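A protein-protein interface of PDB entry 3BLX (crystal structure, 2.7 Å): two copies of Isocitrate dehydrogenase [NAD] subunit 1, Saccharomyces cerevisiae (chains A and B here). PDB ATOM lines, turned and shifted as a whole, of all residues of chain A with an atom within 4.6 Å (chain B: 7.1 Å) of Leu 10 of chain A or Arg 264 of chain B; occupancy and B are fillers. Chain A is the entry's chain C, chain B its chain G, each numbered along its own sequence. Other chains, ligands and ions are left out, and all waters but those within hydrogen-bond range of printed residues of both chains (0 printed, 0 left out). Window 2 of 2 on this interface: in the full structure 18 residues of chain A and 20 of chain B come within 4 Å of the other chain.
The backbone NH (N) of Tyr 104 of chain B lies within hydrogen-bond range of the backbone carbonyl oxygen (O) of Phe 262 of chain B.
No position is printed for both chains.
Of the 12 pairs that touch across the chains among the printed residues, none has its exchanged pair printed and touching as well.
Of chain B, only Arg 264 (3.4 Å) comes within 4 Å of Leu 10 of chain A.
Leu 101 of chain B touches none of the printed residues of chain A.
Printed residues of chain A within 4 Å of Gly 263 of chain B: Tyr 14 (3.99 Å) and Gly 15 (3.0 Å).
Of chain A, only Leu 10 (3.4 Å), Pro 11 (2.7 Å), Lys 13 (3.7 Å), Tyr 14 (3.8 Å), Gly 15 (3.3 Å) and Gly 16 (3.1 Å) come within 4 Å of Arg 264 of chain B.
Printed residues of chain A within 4 Å of Tyr 266 of chain B: Gly 15.
The nearest printed residue of chain B that does not touch Leu 10 of chain A is Asp 265 of chain B (7.7 Å).
Leu 10 of chain A touches Arg 264 of chain B.
CB of Lys 13 of chain A touches NH1 of Arg 264 of chain B, 3.7 Å away.
Tyr 14 of chain A touches Tyr 104 of chain B.
O of Gly 263 of chain B touches C of Tyr 14 of chain A, at 3.99 Å.
Tyr 14 of chain A touches Arg 264 of chain B.
Gly 15 of chain A touches Tyr 266 of chain B (CA to O, 3.5 Å).
Gly 16 of chain A touches Asp 265 of chain B (N to O, 3.8 Å).
Of the 11 printed residues of chain B, 5 touch a printed residue of chain A.
Hydrophobic or aromatic side chains of chain B that line the printed part of chain A: Tyr 104.
Hydrophobic or aromatic side chains of chain A within 4 Å of the printed part of chain B: Leu 10 and Tyr 14.
Among the printed residues, Asp or Glu carboxylates within 4 Å of a Lys or Arg side-chain nitrogen of the other chain: Lys 13 of chain A with Asp 265 of chain B (3.0 Å).
The backbone carbonyl oxygen (O) of Pro 11 of chain A lies within hydrogen-bond range of the guanidinium group (NH1) of Arg 264 of chain B (2.7 Å).
NZ of Lys 13 of chain A lies within salt-bridge range of OD1 of Asp 265 of chain B (3.0 Å).
The backbone NH (N) of Gly 15 of chain A lies within hydrogen-bond range of the backbone carbonyl oxygen (O) of Gly 263 of chain B (3.0 Å).
N of Gly 15 of chain A lies within hydrogen-bond range of O of Arg 264 of chain B (3.3 Å).
The backbone carbonyl oxygen (O) of Arg 264 of chain B sits at hydrogen-bond distance from the backbone NH (N) of Gly 16 of chain A (3.1 Å).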
ATOM      1  N   ARG A   8     -25.965  25.096 -24.302  1.00  0.00           N
ATOM      2  CA  ARG A   8     -25.604  24.419 -25.568  1.00  0.00           C
ATOM      3  C   ARG A   8     -24.827  25.286 -26.609  1.00  0.00           C
ATOM      4  O   ARG A   8     -24.356  24.761 -27.616  1.00  0.00           O
ATOM      5  CB  ARG A   8     -26.851  23.827 -26.251  1.00  0.00           C
ATOM      6  CG  ARG A   8     -27.512  24.815 -27.247  1.00  0.00           C
ATOM      7  CD  ARG A   8     -28.574  24.200 -28.161  1.00  0.00           C
ATOM      8  NE  ARG A   8     -29.866  24.090 -27.483  1.00  0.00           N
ATOM      9  CZ  ARG A   8     -31.036  23.910 -28.097  1.00  0.00           C
ATOM     10  NH1 ARG A   8     -31.088  23.831 -29.427  1.00  0.00           N
ATOM     11  NH2 ARG A   8     -32.158  23.818 -27.382  1.00  0.00           N
ATOM     12  N   THR A   9     -24.725  26.601 -26.412  1.00  0.00           N
ATOM     13  CA  THR A   9     -23.816  27.403 -27.244  1.00  0.00           C
ATOM     14  C   THR A   9     -22.554  27.749 -26.447  1.00  0.00           C
ATOM     15  O   THR A   9     -21.743  28.618 -26.828  1.00  0.00           O
ATOM     16  CB  THR A   9     -24.484  28.671 -27.877  1.00  0.00           C
ATOM     17  OG1 THR A   9     -24.708  29.679 -26.880  1.00  0.00           O
ATOM     18  CG2 THR A   9     -25.790  28.303 -28.549  1.00  0.00           C
ATOM     19  N   LEU A  10     -22.397  27.049 -25.331  1.00  0.00           N
ATOM     20  CA  LEU A  10     -21.170  27.142 -24.575  1.00  0.00           C
ATOM     21  C   LEU A  10     -20.144  26.112 -25.088  1.00  0.00           C
ATOM     22  O   LEU A  10     -20.488  25.109 -25.716  1.00  0.00           O
ATOM     23  CB  LEU A  10     -21.479  26.925 -23.107  1.00  0.00           C
ATOM     24  CG  LEU A  10     -22.363  27.947 -22.372  1.00  0.00           C
ATOM     25  CD1 LEU A  10     -23.211  27.256 -21.309  1.00  0.00           C
ATOM     26  CD2 LEU A  10     -21.525  29.068 -21.737  1.00  0.00           C
ATOM     27  N   PRO A  11     -18.870  26.362 -24.840  1.00  0.00           N
ATOM     28  CA  PRO A  11     -17.898  25.280 -25.010  1.00  0.00           C
ATOM     29  C   PRO A  11     -18.407  23.960 -24.411  1.00  0.00           C
ATOM     30  O   PRO A  11     -19.128  23.950 -23.447  1.00  0.00           O
ATOM     31  CB  PRO A  11     -16.694  25.763 -24.194  1.00  0.00           C
ATOM     32  CG  PRO A  11     -16.826  27.221 -24.114  1.00  0.00           C
ATOM     33  CD  PRO A  11     -18.302  27.555 -24.198  1.00  0.00           C
ATOM     34  N   LYS A  12     -18.005  22.849 -24.997  1.00  0.00           N
ATOM     35  CA  LYS A  12     -18.404  21.521 -24.565  1.00  0.00           C
ATOM     36  C   LYS A  12     -17.647  21.211 -23.276  1.00  0.00           C
ATOM     37  O   LYS A  12     -16.419  21.313 -23.219  1.00  0.00           O
ATOM     38  CB  LYS A  12     -18.086  20.495 -25.665  1.00  0.00           C
ATOM     39  CG  LYS A  12     -18.542  19.085 -25.363  1.00  0.00           C
ATOM     40  CD  LYS A  12     -18.192  18.093 -26.485  1.00  0.00           C
ATOM     41  CE  LYS A  12     -18.919  18.418 -27.773  1.00  0.00           C
ATOM     42  NZ  LYS A  12     -20.390  18.302 -27.727  1.00  0.00           N
ATOM     43  N   LYS A  13     -18.392  20.873 -22.228  1.00  0.00           N
ATOM     44  CA  LYS A  13     -17.788  20.714 -20.927  1.00  0.00           C
ATOM     45  C   LYS A  13     -18.536  19.667 -20.104  1.00  0.00           C
ATOM     46  O   LYS A  13     -19.754  19.724 -19.933  1.00  0.00           O
ATOM     47  CB  LYS A  13     -17.764  22.065 -20.252  1.00  0.00           C
ATOM     48  CG  LYS A  13     -16.848  22.200 -19.109  1.00  0.00           C
ATOM     49  CD  LYS A  13     -17.208  23.459 -18.361  1.00  0.00           C
ATOM     50  CE  LYS A  13     -16.333  23.674 -17.129  1.00  0.00           C
ATOM     51  NZ  LYS A  13     -16.721  24.960 -16.481  1.00  0.00           N
ATOM     52  N   TYR A  14     -17.800  18.685 -19.615  1.00  0.00           N
ATOM     53  CA  TYR A  14     -18.391  17.642 -18.791  1.00  0.00           C
ATOM     54  C   TYR A  14     -17.596  17.518 -17.530  1.00  0.00           C
ATOM     55  O   TYR A  14     -16.357  17.395 -17.574  1.00  0.00           O
ATOM     56  CB  TYR A  14     -18.426  16.303 -19.517  1.00  0.00           C
ATOM     57  CG  TYR A  14     -19.338  16.311 -20.701  1.00  0.00           C
ATOM     58  CD1 TYR A  14     -18.854  16.204 -21.981  1.00  0.00           C
ATOM     59  CD2 TYR A  14     -20.701  16.456 -20.529  1.00  0.00           C
ATOM     60  CE1 TYR A  14     -19.732  16.220 -23.078  1.00  0.00           C
ATOM     61  CE2 TYR A  14     -21.565  16.482 -21.588  1.00  0.00           C
ATOM     62  CZ  TYR A  14     -21.087  16.368 -22.859  1.00  0.00           C
ATOM     63  OH  TYR A  14     -21.992  16.380 -23.887  1.00  0.00           O
ATOM     64  N   GLY A  15     -18.321  17.569 -16.406  1.00  0.00           N
ATOM     65  CA  GLY A  15     -17.730  17.502 -15.091  1.00  0.00           C
ATOM     66  C   GLY A  15     -16.518  18.388 -14.904  1.00  0.00           C
ATOM     67  O   GLY A  15     -15.544  18.002 -14.293  1.00  0.00           O
ATOM     68  N   GLY A  16     -16.526  19.581 -15.469  1.00  0.00           N
ATOM     69  CA  GLY A  16     -15.348  20.408 -15.329  1.00  0.00           C
ATOM     70  C   GLY A  16     -14.245  20.193 -16.349  1.00  0.00           C
ATOM     71  O   GLY A  16     -13.246  20.919 -16.297  1.00  0.00           O
ATOM     72  N   LYS A  74     -17.007  24.030 -30.165  1.00  0.00           N
ATOM     73  CA  LYS A  74     -16.990  25.502 -30.155  1.00  0.00           C
ATOM     74  C   LYS A  74     -15.633  26.185 -29.996  1.00  0.00           C
ATOM     75  O   LYS A  74     -15.495  27.314 -30.384  1.00  0.00           O
ATOM     76  CB  LYS A  74     -17.960  26.064 -29.135  1.00  0.00           C
ATOM     77  CG  LYS A  74     -19.315  25.390 -29.080  1.00  0.00           C
ATOM     78  CD  LYS A  74     -20.048  25.507 -30.339  1.00  0.00           C
ATOM     79  CE  LYS A  74     -21.517  25.270 -30.158  1.00  0.00           C
ATOM     80  NZ  LYS A  74     -21.798  23.910 -29.631  1.00  0.00           N
ATOM     81  N   LEU B 101     -27.380  21.379  -8.547  1.00  0.00           N
ATOM     82  CA  LEU B 101     -26.126  21.234  -9.273  1.00  0.00           C
ATOM     83  C   LEU B 101     -26.352  20.900 -10.757  1.00  0.00           C
ATOM     84  O   LEU B 101     -25.443  20.913 -11.559  1.00  0.00           O
ATOM     85  CB  LEU B 101     -25.234  20.199  -8.604  1.00  0.00           C
ATOM     86  CG  LEU B 101     -24.717  20.570  -7.220  1.00  0.00           C
ATOM     87  CD1 LEU B 101     -23.620  19.592  -6.845  1.00  0.00           C
ATOM     88  CD2 LEU B 101     -24.186  21.963  -7.245  1.00  0.00           C
ATOM     89  N   ASP B 102     -27.591  20.638 -11.106  1.00  0.00           N
ATOM     90  CA  ASP B 102     -27.921  20.257 -12.439  1.00  0.00           C
ATOM     91  C   ASP B 102     -27.028  19.134 -12.958  1.00  0.00           C
ATOM     92  O   ASP B 102     -26.513  19.207 -14.066  1.00  0.00           O
ATOM     93  CB  ASP B 102     -27.844  21.463 -13.352  1.00  0.00           C
ATOM     94  CG  ASP B 102     -28.667  21.266 -14.650  1.00  0.00           C
ATOM     95  OD1 ASP B 102     -29.655  20.471 -14.651  1.00  0.00           O
ATOM     96  OD2 ASP B 102     -28.317  21.917 -15.661  1.00  0.00           O
ATOM     97  N   ILE B 103     -26.851  18.095 -12.157  1.00  0.00           N
ATOM     98  CA  ILE B 103     -26.185  16.883 -12.588  1.00  0.00           C
ATOM     99  C   ILE B 103     -27.218  16.015 -13.296  1.00  0.00           C
ATOM    100  O   ILE B 103     -28.120  15.493 -12.680  1.00  0.00           O
ATOM    101  CB  ILE B 103     -25.587  16.175 -11.397  1.00  0.00           C
ATOM    102  CG1 ILE B 103     -24.522  17.064 -10.783  1.00  0.00           C
ATOM    103  CG2 ILE B 103     -24.992  14.847 -11.746  1.00  0.00           C
ATOM    104  CD1 ILE B 103     -23.957  16.507  -9.499  1.00  0.00           C
ATOM    105  N   TYR B 104     -27.078  15.877 -14.608  1.00  0.00           N
ATOM    106  CA  TYR B 104     -28.181  15.412 -15.434  1.00  0.00           C
ATOM    107  C   TYR B 104     -27.949  14.056 -16.054  1.00  0.00           C
ATOM    108  O   TYR B 104     -28.845  13.521 -16.667  1.00  0.00           O
ATOM    109  CB  TYR B 104     -28.463  16.433 -16.554  1.00  0.00           C
ATOM    110  CG  TYR B 104     -27.309  16.683 -17.514  1.00  0.00           C
ATOM    111  CD1 TYR B 104     -26.438  17.723 -17.304  1.00  0.00           C
ATOM    112  CD2 TYR B 104     -27.093  15.870 -18.637  1.00  0.00           C
ATOM    113  CE1 TYR B 104     -25.386  17.958 -18.171  1.00  0.00           C
ATOM    114  CE2 TYR B 104     -26.023  16.103 -19.516  1.00  0.00           C
ATOM    115  CZ  TYR B 104     -25.176  17.159 -19.273  1.00  0.00           C
ATOM    116  OH  TYR B 104     -24.101  17.479 -20.086  1.00  0.00           O
ATOM    117  N   ARG B 161     -29.341  17.372 -24.522  1.00  0.00           N
ATOM    118  CA  ARG B 161     -28.192  17.258 -23.617  1.00  0.00           C
ATOM    119  C   ARG B 161     -27.794  15.823 -23.413  1.00  0.00           C
ATOM    120  O   ARG B 161     -26.609  15.475 -23.551  1.00  0.00           O
ATOM    121  CB  ARG B 161     -28.531  17.811 -22.252  1.00  0.00           C
ATOM    122  CG  ARG B 161     -27.870  19.081 -21.875  1.00  0.00           C
ATOM    123  CD  ARG B 161     -27.786  19.212 -20.375  1.00  0.00           C
ATOM    124  NE  ARG B 161     -29.011  18.826 -19.651  1.00  0.00           N
ATOM    125  CZ  ARG B 161     -29.403  19.450 -18.540  1.00  0.00           C
ATOM    126  NH1 ARG B 161     -28.691  20.474 -18.110  1.00  0.00           N
ATOM    127  NH2 ARG B 161     -30.498  19.096 -17.881  1.00  0.00           N
ATOM    128  N   PHE B 262     -22.772  13.091 -13.977  1.00  0.00           N
ATOM    129  CA  PHE B 262     -22.166  14.296 -14.539  1.00  0.00           C
ATOM    130  C   PHE B 262     -23.150  15.405 -14.735  1.00  0.00           C
ATOM    131  O   PHE B 262     -24.288  15.178 -15.143  1.00  0.00           O
ATOM    132  CB  PHE B 262     -21.510  14.012 -15.897  1.00  0.00           C
ATOM    133  CG  PHE B 262     -20.363  13.046 -15.832  1.00  0.00           C
ATOM    134  CD1 PHE B 262     -20.575  11.700 -15.997  1.00  0.00           C
ATOM    135  CD2 PHE B 262     -19.084  13.488 -15.633  1.00  0.00           C
ATOM    136  CE1 PHE B 262     -19.540  10.819 -15.954  1.00  0.00           C
ATOM    137  CE2 PHE B 262     -18.040  12.602 -15.578  1.00  0.00           C
ATOM    138  CZ  PHE B 262     -18.271  11.262 -15.731  1.00  0.00           C
ATOM    139  N   GLY B 263     -22.698  16.608 -14.433  1.00  0.00           N
ATOM    140  CA  GLY B 263     -23.331  17.809 -14.912  1.00  0.00           C
ATOM    141  C   GLY B 263     -22.331  18.560 -15.760  1.00  0.00           C
ATOM    142  O   GLY B 263     -21.254  18.063 -16.032  1.00  0.00           O
ATOM    143  N   ARG B 264     -22.653  19.769 -16.178  1.00  0.00           N
ATOM    144  CA  ARG B 264     -21.663  20.567 -16.891  1.00  0.00           C
ATOM    145  C   ARG B 264     -20.449  20.874 -15.993  1.00  0.00           C
ATOM    146  O   ARG B 264     -19.309  20.698 -16.375  1.00  0.00           O
ATOM    147  CB  ARG B 264     -22.294  21.864 -17.397  1.00  0.00           C
ATOM    148  CG  ARG B 264     -21.362  22.704 -18.176  1.00  0.00           C
ATOM    149  CD  ARG B 264     -21.992  23.938 -18.704  1.00  0.00           C
ATOM    150  NE  ARG B 264     -20.970  24.873 -19.157  1.00  0.00           N
ATOM    151  CZ  ARG B 264     -20.408  24.850 -20.359  1.00  0.00           C
ATOM    152  NH1 ARG B 264     -20.766  23.936 -21.241  1.00  0.00           N
ATOM    153  NH2 ARG B 264     -19.483  25.743 -20.671  1.00  0.00           N
ATOM    154  N   ASP B 265     -20.694  21.333 -14.771  1.00  0.00           N
ATOM    155  CA  ASP B 265     -19.606  21.843 -13.931  1.00  0.00           C
ATOM    156  C   ASP B 265     -19.184  20.849 -12.878  1.00  0.00           C
ATOM    157  O   ASP B 265     -18.114  21.007 -12.302  1.00  0.00           O
ATOM    158  CB  ASP B 265     -19.992  23.173 -13.270  1.00  0.00           C
ATOM    159  CG  ASP B 265     -20.253  24.292 -14.300  1.00  0.00           C
ATOM    160  OD1 ASP B 265     -19.433  24.442 -15.238  1.00  0.00           O
ATOM    161  OD2 ASP B 265     -21.271  25.029 -14.165  1.00  0.00           O
ATOM    162  N   TYR B 266     -19.993  19.815 -12.646  1.00  0.00           N
ATOM    163  CA  TYR B 266     -19.740  18.936 -11.521  1.00  0.00           C
ATOM    164  C   TYR B 266     -19.730  17.485 -11.923  1.00  0.00           C
ATOM    165  O   TYR B 266     -20.355  17.088 -12.878  1.00  0.00           O
ATOM    166  CB  TYR B 266     -20.790  19.167 -10.426  1.00  0.00           C
ATOM    167  CG  TYR B 266     -20.990  20.616 -10.094  1.00  0.00           C
ATOM    168  CD1 TYR B 266     -22.094  21.320 -10.572  1.00  0.00           C
ATOM    169  CD2 TYR B 266     -20.073  21.279  -9.305  1.00  0.00           C
ATOM    170  CE1 TYR B 266     -22.268  22.660 -10.272  1.00  0.00           C
ATOM    171  CE2 TYR B 266     -20.245  22.614  -8.969  1.00  0.00           C
ATOM    172  CZ  TYR B 266     -21.342  23.312  -9.459  1.00  0.00           C
ATOM    173  OH  TYR B 266     -21.491  24.659  -9.147  1.00  0.00           O
ATOM    174  N   ALA B 267     -19.044  16.681 -11.138  1.00  0.00           N
ATOM    175  CA  ALA B 267     -19.055  15.239 -11.313  1.00  0.00           C
ATOM    176  C   ALA B 267     -19.050  14.575  -9.949  1.00  0.00           C
ATOM    177  O   ALA B 267     -18.267  14.953  -9.073  1.00  0.00           O
ATOM    178  CB  ALA B 267     -17.838  14.808 -12.098  1.00  0.00           C
